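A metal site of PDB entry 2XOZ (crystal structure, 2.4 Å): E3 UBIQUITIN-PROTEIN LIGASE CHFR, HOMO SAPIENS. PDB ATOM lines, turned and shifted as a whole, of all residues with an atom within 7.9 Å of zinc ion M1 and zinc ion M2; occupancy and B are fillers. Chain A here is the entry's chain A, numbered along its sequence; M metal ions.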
ATOM      1  N   ARG A  26      -5.606 -18.347   7.394  1.00  0.00           N
ATOM      2  CA  ARG A  26      -4.727 -17.363   6.739  1.00  0.00           C
ATOM      3  C   ARG A  26      -3.338 -17.900   6.368  1.00  0.00           C
ATOM      4  O   ARG A  26      -2.740 -17.448   5.392  1.00  0.00           O
ATOM      5  CB  ARG A  26      -4.532 -16.143   7.652  1.00  0.00           C
ATOM      6  CG  ARG A  26      -5.682 -15.162   7.731  1.00  0.00           C
ATOM      7  CD  ARG A  26      -5.233 -13.873   8.406  1.00  0.00           C
ATOM      8  NE  ARG A  26      -6.213 -13.442   9.398  1.00  0.00           N
ATOM      9  CZ  ARG A  26      -6.055 -12.385  10.200  1.00  0.00           C
ATOM     10  NH1 ARG A  26      -4.949 -11.663  10.128  1.00  0.00           N
ATOM     11  NH2 ARG A  26      -7.015 -12.061  11.081  1.00  0.00           N
ATOM     12  N   LEU A  81      -9.544 -22.089  17.342  1.00  0.00           N
ATOM     13  CA  LEU A  81     -10.458 -21.024  16.965  1.00  0.00           C
ATOM     14  C   LEU A  81     -10.323 -19.855  17.932  1.00  0.00           C
ATOM     15  O   LEU A  81     -10.480 -20.032  19.141  1.00  0.00           O
ATOM     16  CB  LEU A  81     -11.896 -21.546  16.960  1.00  0.00           C
ATOM     17  CG  LEU A  81     -12.185 -22.675  15.959  1.00  0.00           C
ATOM     18  CD1 LEU A  81     -13.652 -23.043  15.943  1.00  0.00           C
ATOM     19  CD2 LEU A  81     -11.735 -22.266  14.582  1.00  0.00           C
ATOM     20  N   CYS A  82     -10.019 -18.676  17.395  1.00  0.00           N
ATOM     21  CA  CYS A  82     -10.030 -17.458  18.185  1.00  0.00           C
ATOM     22  C   CYS A  82     -11.380 -17.319  18.864  1.00  0.00           C
ATOM     23  O   CYS A  82     -12.414 -17.431  18.218  1.00  0.00           O
ATOM     24  CB  CYS A  82      -9.781 -16.213  17.307  1.00  0.00           C
ATOM     25  SG  CYS A  82     -10.092 -14.655  18.176  1.00  0.00           S
ATOM     26  N   THR A  83     -11.360 -17.066  20.178  1.00  0.00           N
ATOM     27  CA  THR A  83     -12.569 -16.962  20.985  1.00  0.00           C
ATOM     28  C   THR A  83     -13.420 -15.737  20.607  1.00  0.00           C
ATOM     29  O   THR A  83     -14.629 -15.683  20.868  1.00  0.00           O
ATOM     30  CB  THR A  83     -12.200 -16.892  22.487  1.00  0.00           C
ATOM     31  OG1 THR A  83     -11.394 -18.016  22.827  1.00  0.00           O
ATOM     32  CG2 THR A  83     -13.444 -16.853  23.387  1.00  0.00           C
ATOM     33  N   CYS A  84     -12.784 -14.736  19.997  1.00  0.00           N
ATOM     34  CA  CYS A  84     -13.472 -13.491  19.660  1.00  0.00           C
ATOM     35  C   CYS A  84     -14.142 -13.574  18.294  1.00  0.00           C
ATOM     36  O   CYS A  84     -15.351 -13.368  18.180  1.00  0.00           O
ATOM     37  CB  CYS A  84     -12.499 -12.304  19.706  1.00  0.00           C
ATOM     38  SG  CYS A  84     -13.149 -10.789  18.969  1.00  0.00           S
ATOM     39  N   CYS A  85     -13.362 -13.862  17.261  1.00  0.00           N
ATOM     40  CA  CYS A  85     -13.868 -13.850  15.894  1.00  0.00           C
ATOM     41  C   CYS A  85     -14.216 -15.243  15.314  1.00  0.00           C
ATOM     42  O   CYS A  85     -14.727 -15.332  14.190  1.00  0.00           O
ATOM     43  CB  CYS A  85     -12.873 -13.141  14.984  1.00  0.00           C
ATOM     44  SG  CYS A  85     -11.342 -14.066  14.726  1.00  0.00           S
ATOM     45  N   PHE A  86     -13.947 -16.303  16.062  1.00  0.00           N
ATOM     46  CA  PHE A  86     -14.208 -17.681  15.609  1.00  0.00           C
ATOM     47  C   PHE A  86     -13.413 -18.152  14.369  1.00  0.00           C
ATOM     48  O   PHE A  86     -13.723 -19.204  13.795  1.00  0.00           O
ATOM     49  CB  PHE A  86     -15.717 -17.929  15.382  1.00  0.00           C
ATOM     50  CG  PHE A  86     -16.615 -17.254  16.399  1.00  0.00           C
ATOM     51  CD1 PHE A  86     -16.650 -17.679  17.725  1.00  0.00           C
ATOM     52  CD2 PHE A  86     -17.416 -16.183  16.024  1.00  0.00           C
ATOM     53  CE1 PHE A  86     -17.467 -17.041  18.655  1.00  0.00           C
ATOM     54  CE2 PHE A  86     -18.243 -15.543  16.953  1.00  0.00           C
ATOM     55  CZ  PHE A  86     -18.259 -15.979  18.268  1.00  0.00           C
ATOM     56  N   GLN A  87     -12.404 -17.381  13.958  1.00  0.00           N
ATOM     57  CA  GLN A  87     -11.543 -17.777  12.829  1.00  0.00           C
ATOM     58  C   GLN A  87     -10.412 -18.690  13.310  1.00  0.00           C
ATOM     59  O   GLN A  87      -9.859 -18.474  14.379  1.00  0.00           O
ATOM     60  CB  GLN A  87     -10.951 -16.550  12.112  1.00  0.00           C
ATOM     61  CG  GLN A  87     -11.990 -15.595  11.515  1.00  0.00           C
ATOM     62  CD  GLN A  87     -12.978 -16.330  10.615  1.00  0.00           C
ATOM     63  OE1 GLN A  87     -12.614 -16.792   9.527  1.00  0.00           O
ATOM     64  NE2 GLN A  87     -14.230 -16.442  11.065  1.00  0.00           N
ATOM     65  N   PRO A  88     -10.060 -19.717  12.510  1.00  0.00           N
ATOM     66  CA  PRO A  88      -8.973 -20.620  12.906  1.00  0.00           C
ATOM     67  C   PRO A  88      -7.601 -19.973  12.763  1.00  0.00           C
ATOM     68  O   PRO A  88      -7.354 -19.184  11.861  1.00  0.00           O
ATOM     69  CB  PRO A  88      -9.103 -21.762  11.916  1.00  0.00           C
ATOM     70  CG  PRO A  88      -9.676 -21.099  10.685  1.00  0.00           C
ATOM     71  CD  PRO A  88     -10.692 -20.137  11.240  1.00  0.00           C
ATOM     72  N   MET A  89      -6.715 -20.306  13.698  1.00  0.00           N
ATOM     73  CA  MET A  89      -5.321 -19.905  13.634  1.00  0.00           C
ATOM     74  C   MET A  89      -4.519 -21.134  13.975  1.00  0.00           C
ATOM     75  O   MET A  89      -5.035 -22.073  14.572  1.00  0.00           O
ATOM     76  CB  MET A  89      -5.029 -18.771  14.616  1.00  0.00           C
ATOM     77  CG  MET A  89      -5.305 -19.138  16.062  1.00  0.00           C
ATOM     78  SD  MET A  89      -5.087 -17.751  17.181  1.00  0.00           S
ATOM     79  CE  MET A  89      -5.753 -18.433  18.681  1.00  0.00           C
ATOM     80  N   PRO A 113      -8.232 -18.998  23.753  1.00  0.00           N
ATOM     81  CA  PRO A 113      -7.355 -18.454  22.702  1.00  0.00           C
ATOM     82  C   PRO A 113      -7.937 -17.243  21.969  1.00  0.00           C
ATOM     83  O   PRO A 113      -9.138 -17.182  21.701  1.00  0.00           O
ATOM     84  CB  PRO A 113      -7.178 -19.632  21.740  1.00  0.00           C
ATOM     85  CG  PRO A 113      -8.425 -20.462  21.915  1.00  0.00           C
ATOM     86  CD  PRO A 113      -9.007 -20.157  23.273  1.00  0.00           C
ATOM     87  N   PHE A 114      -7.060 -16.293  21.648  1.00  0.00           N
ATOM     88  CA  PHE A 114      -7.421 -15.122  20.850  1.00  0.00           C
ATOM     89  C   PHE A 114      -6.369 -14.850  19.791  1.00  0.00           C
ATOM     90  O   PHE A 114      -5.173 -15.033  20.014  1.00  0.00           O
ATOM     91  CB  PHE A 114      -7.612 -13.916  21.757  1.00  0.00           C
ATOM     92  CG  PHE A 114      -8.717 -14.084  22.767  1.00  0.00           C
ATOM     93  CD1 PHE A 114      -9.965 -13.552  22.523  1.00  0.00           C
ATOM     94  CD2 PHE A 114      -8.492 -14.799  23.931  1.00  0.00           C
ATOM     95  CE1 PHE A 114     -10.985 -13.716  23.449  1.00  0.00           C
ATOM     96  CE2 PHE A 114      -9.512 -14.963  24.857  1.00  0.00           C
ATOM     97  CZ  PHE A 114     -10.759 -14.422  24.616  1.00  0.00           C
ATOM     98  N   CYS A 115      -6.804 -14.409  18.614  1.00  0.00           N
ATOM     99  CA  CYS A 115      -5.858 -14.257  17.512  1.00  0.00           C
ATOM    100  C   CYS A 115      -5.193 -12.865  17.421  1.00  0.00           C
ATOM    101  O   CYS A 115      -4.275 -12.662  16.622  1.00  0.00           O
ATOM    102  CB  CYS A 115      -6.534 -14.590  16.179  1.00  0.00           C
ATOM    103  SG  CYS A 115      -7.544 -13.236  15.499  1.00  0.00           S
ATOM    104  N   HIS A 116      -5.636 -11.911  18.223  1.00  0.00           N
ATOM    105  CA  HIS A 116      -5.267 -10.526  17.958  1.00  0.00           C
ATOM    106  C   HIS A 116      -3.772 -10.179  17.961  1.00  0.00           C
ATOM    107  O   HIS A 116      -3.303  -9.448  17.093  1.00  0.00           O
ATOM    108  CB  HIS A 116      -5.994  -9.540  18.880  1.00  0.00           C
ATOM    109  CG  HIS A 116      -5.776  -8.129  18.483  1.00  0.00           C
ATOM    110  ND1 HIS A 116      -6.299  -7.588  17.327  1.00  0.00           N
ATOM    111  CD2 HIS A 116      -5.039  -7.137  19.048  1.00  0.00           C
ATOM    112  CE1 HIS A 116      -5.925  -6.332  17.213  1.00  0.00           C
ATOM    113  NE2 HIS A 116      -5.157  -6.030  18.254  1.00  0.00           N
ATOM    114  N   LEU A 117      -3.029 -10.648  18.959  1.00  0.00           N
ATOM    115  CA  LEU A 117      -1.597 -10.363  19.022  1.00  0.00           C
ATOM    116  C   LEU A 117      -0.852 -11.187  18.003  1.00  0.00           C
ATOM    117  O   LEU A 117       0.226 -10.798  17.542  1.00  0.00           O
ATOM    118  CB  LEU A 117      -1.032 -10.664  20.417  1.00  0.00           C
ATOM    119  CG  LEU A 117      -1.469  -9.650  21.477  1.00  0.00           C
ATOM    120  CD1 LEU A 117      -0.878  -9.992  22.821  1.00  0.00           C
ATOM    121  CD2 LEU A 117      -1.039  -8.251  21.033  1.00  0.00           C
ATOM    122  N   TRP A 119      -1.847 -12.144  14.818  1.00  0.00           N
ATOM    123  CA  TRP A 119      -1.927 -11.620  13.456  1.00  0.00           C
ATOM    124  C   TRP A 119      -3.011 -10.572  13.206  1.00  0.00           C
ATOM    125  O   TRP A 119      -3.314 -10.263  12.066  1.00  0.00           O
ATOM    126  CB  TRP A 119      -2.056 -12.764  12.435  1.00  0.00           C
ATOM    127  CG  TRP A 119      -3.319 -13.590  12.537  1.00  0.00           C
ATOM    128  CD1 TRP A 119      -4.474 -13.239  13.157  1.00  0.00           C
ATOM    129  CD2 TRP A 119      -3.543 -14.892  11.952  1.00  0.00           C
ATOM    130  NE1 TRP A 119      -5.407 -14.247  13.019  1.00  0.00           N
ATOM    131  CE2 TRP A 119      -4.855 -15.265  12.282  1.00  0.00           C
ATOM    132  CE3 TRP A 119      -2.767 -15.764  11.192  1.00  0.00           C
ATOM    133  CZ2 TRP A 119      -5.410 -16.484  11.878  1.00  0.00           C
ATOM    134  CZ3 TRP A 119      -3.311 -16.974  10.792  1.00  0.00           C
ATOM    135  CH2 TRP A 119      -4.612 -17.332  11.137  1.00  0.00           C
ATOM    136  N   GLY A 120      -3.573 -10.015  14.271  1.00  0.00           N
ATOM    137  CA  GLY A 120      -4.549  -8.949  14.129  1.00  0.00           C
ATOM    138  C   GLY A 120      -5.930  -9.517  13.866  1.00  0.00           C
ATOM    139  O   GLY A 120      -6.155 -10.193  12.863  1.00  0.00           O
ATOM    140  N   CYS A 121      -6.833  -9.279  14.800  1.00  0.00           N
ATOM    141  CA  CYS A 121      -8.178  -9.820  14.715  1.00  0.00           C
ATOM    142  C   CYS A 121      -9.101  -8.736  14.165  1.00  0.00           C
ATOM    143  O   CYS A 121      -8.852  -7.542  14.357  1.00  0.00           O
ATOM    144  CB  CYS A 121      -8.635 -10.267  16.112  1.00  0.00           C
ATOM    145  SG  CYS A 121     -10.345 -10.805  16.245  1.00  0.00           S
ATOM    146  N   THR A 122     -10.163  -9.136  13.477  1.00  0.00           N
ATOM    147  CA  THR A 122     -11.124  -8.163  12.966  1.00  0.00           C
ATOM    148  C   THR A 122     -12.554  -8.654  13.106  1.00  0.00           C
ATOM    149  O   THR A 122     -12.903  -9.725  12.648  1.00  0.00           O
ATOM    150  CB  THR A 122     -10.861  -7.833  11.477  1.00  0.00           C
ATOM    151  OG1 THR A 122      -9.545  -7.290  11.352  1.00  0.00           O
ATOM    152  CG2 THR A 122     -11.887  -6.828  10.959  1.00  0.00           C
ATOM    153  N   ARG A 123     -13.371  -7.833  13.733  1.00  0.00           N
ATOM    154  CA  ARG A 123     -14.783  -8.119  13.880  1.00  0.00           C
ATOM    155  C   ARG A 123     -15.410  -6.849  14.400  1.00  0.00           C
ATOM    156  O   ARG A 123     -14.807  -6.145  15.216  1.00  0.00           O
ATOM    157  CB  ARG A 123     -15.024  -9.256  14.894  1.00  0.00           C
ATOM    158  CG  ARG A 123     -16.502  -9.553  15.105  1.00  0.00           C
ATOM    159  CD  ARG A 123     -16.784 -10.730  16.020  1.00  0.00           C
ATOM    160  NE  ARG A 123     -16.352 -10.473  17.393  1.00  0.00           N
ATOM    161  CZ  ARG A 123     -17.043  -9.752  18.274  1.00  0.00           C
ATOM    162  NH1 ARG A 123     -18.201  -9.192  17.932  1.00  0.00           N
ATOM    163  NH2 ARG A 123     -16.565  -9.574  19.504  1.00  0.00           N
ATOM    164  N   GLY A 125     -17.174  -4.987  16.862  1.00  0.00           N
ATOM    165  CA  GLY A 125     -17.352  -5.236  18.288  1.00  0.00           C
ATOM    166  C   GLY A 125     -16.042  -5.522  18.992  1.00  0.00           C
ATOM    167  O   GLY A 125     -15.960  -5.431  20.224  1.00  0.00           O
ATOM    168  N   CYS A 126     -15.020  -5.864  18.216  1.00  0.00           N
ATOM    169  CA  CYS A 126     -13.693  -6.163  18.742  1.00  0.00           C
ATOM    170  C   CYS A 126     -12.824  -4.907  18.631  1.00  0.00           C
ATOM    171  O   CYS A 126     -12.671  -4.347  17.551  1.00  0.00           O
ATOM    172  CB  CYS A 126     -13.064  -7.355  17.993  1.00  0.00           C
ATOM    173  SG  CYS A 126     -11.267  -7.594  18.182  1.00  0.00           S
ATOM    174  N   TYR A 127     -12.274  -4.474  19.751  1.00  0.00           N
ATOM    175  CA  TYR A 127     -11.461  -3.271  19.809  1.00  0.00           C
ATOM    176  C   TYR A 127      -9.990  -3.634  19.703  1.00  0.00           C
ATOM    177  O   TYR A 127      -9.126  -2.752  19.654  1.00  0.00           O
ATOM    178  CB  TYR A 127     -11.692  -2.560  21.135  1.00  0.00           C
ATOM    179  CG  TYR A 127     -13.146  -2.353  21.480  1.00  0.00           C
ATOM    180  CD1 TYR A 127     -14.002  -1.712  20.592  1.00  0.00           C
ATOM    181  CD2 TYR A 127     -13.653  -2.792  22.697  1.00  0.00           C
ATOM    182  CE1 TYR A 127     -15.334  -1.511  20.905  1.00  0.00           C
ATOM    183  CE2 TYR A 127     -14.999  -2.611  23.013  1.00  0.00           C
ATOM    184  CZ  TYR A 127     -15.842  -1.958  22.110  1.00  0.00           C
ATOM    185  OH  TYR A 127     -17.173  -1.754  22.412  1.00  0.00           O
ATOM    186  N   GLY A 128      -9.727  -4.938  19.673  1.00  0.00           N
ATOM    187  CA  GLY A 128      -8.390  -5.490  19.909  1.00  0.00           C
ATOM    188  C   GLY A 128      -8.433  -6.355  21.163  1.00  0.00           C
ATOM    189  O   GLY A 128      -8.191  -5.883  22.277  1.00  0.00           O
ATOM    190  N   CYS A 129      -8.705  -7.648  20.962  1.00  0.00           N
ATOM    191  CA  CYS A 129      -9.244  -8.529  21.979  1.00  0.00           C
ATOM    192  C   CYS A 129      -8.223  -9.214  22.879  1.00  0.00           C
ATOM    193  O   CYS A 129      -8.587  -9.989  23.744  1.00  0.00           O
ATOM    194  CB  CYS A 129     -10.119  -9.607  21.305  1.00  0.00           C
ATOM    195  SG  CYS A 129      -9.304 -10.546  19.967  1.00  0.00           S
ATOM    196  N   LEU A 130      -6.939  -8.939  22.645  1.00  0.00           N
ATOM    197  CA  LEU A 130      -5.860  -9.446  23.485  1.00  0.00           C
ATOM    198  C   LEU A 130      -4.776  -8.396  23.555  1.00  0.00           C
ATOM    199  O   LEU A 130      -4.302  -7.908  22.547  1.00  0.00           O
ATOM    200  CB  LEU A 130      -5.288 -10.761  22.927  1.00  0.00           C
ATOM    201  CG  LEU A 130      -4.412 -11.600  23.875  1.00  0.00           C
ATOM    202  CD1 LEU A 130      -5.252 -12.213  25.003  1.00  0.00           C
ATOM    203  CD2 LEU A 130      -3.626 -12.690  23.107  1.00  0.00           C
ATOM    204  N   TYR A 199     -10.275  -8.887  26.186  1.00  0.00           N
ATOM    205  CA  TYR A 199     -11.262  -7.842  26.412  1.00  0.00           C
ATOM    206  C   TYR A 199     -12.131  -8.115  27.644  1.00  0.00           C
ATOM    207  O   TYR A 199     -12.307  -7.254  28.507  1.00  0.00           O
ATOM    208  CB  TYR A 199     -12.162  -7.705  25.181  1.00  0.00           C
ATOM    209  CG  TYR A 199     -13.388  -6.889  25.499  1.00  0.00           C
ATOM    210  CD1 TYR A 199     -13.294  -5.516  25.644  1.00  0.00           C
ATOM    211  CD2 TYR A 199     -14.624  -7.492  25.687  1.00  0.00           C
ATOM    212  CE1 TYR A 199     -14.406  -4.754  25.956  1.00  0.00           C
ATOM    213  CE2 TYR A 199     -15.746  -6.727  25.990  1.00  0.00           C
ATOM    214  CZ  TYR A 199     -15.621  -5.355  26.126  1.00  0.00           C
ATOM    215  OH  TYR A 199     -16.721  -4.583  26.432  1.00  0.00           O
HETATM  216 ZN    ZN M   1     -11.060 -10.012  18.395  1.00  0.00          ZN
HETATM  217 ZN    ZN M   2      -9.719 -13.199  16.232  1.00  0.00          ZN
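SG of Cys 115 sits close to NE1 of Trp 119. SG of Cys 82 sits close to N of Cys 84, at 3.3 Å. The backbone carbonyl oxygen (O) of Cys 84 sits at hydrogen-bond distance from the guanidinium group (NE) of Arg 123 (3.2 Å). The backbone carbonyl oxygen (O) of Cys 85 lies within hydrogen-bond range of the side-chain amide nitrogen (NE2) of Gln 87 (3.4 Å). N of Cys 121 sits at hydrogen-bond distance from ND1 of His 116. The backbone carbonyl oxygen of Cys 129 is in hydrogen-bond range of the backbone NH of Tyr 199 (3.2 Å). The side-chain sulfur (SG) of Cys 126 sits close to the backbone NH (N) of Gly 128, at 3.4 Å. O of Gln 87 lies within hydrogen-bond range of N of Cys 82, at 3.0 Å.
Four residues have an atom within 4 Å of zinc ion M1: Cys 84, Cys 121, Cys 126 and Cys 129. Along chain A the residues within 4 Å of zinc ion M1 span positions 84 to 129.
The side-chain sulfur (SG) of Cys 115 is bound to zinc ion M2 (2.3 Å). Zinc ion M2 is bound by SG of Cys 85 (2.4 Å). SG of Cys 82 binds zinc ion M2. SG of Cys 121 is bound to zinc ion M2 (2.5 Å).
Within 4 Å of zinc ion M2: Cys 82, Cys 85, Cys 115 and Cys 121. The nearest printed residue that does not touch zinc ion M2 is Cys 84 (4.5 Å).
Zinc ion M1 is bound by the side-chain sulfur (SG) of Cys 84, at 2.3 Å. Zinc ion M1 is bound by SG of Cys 121 (2.4 Å). Zinc ion M1 is bound by SG of Cys 129, 2.4 Å away. SG of Cys 126 binds zinc ion M1 (2.4 Å).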
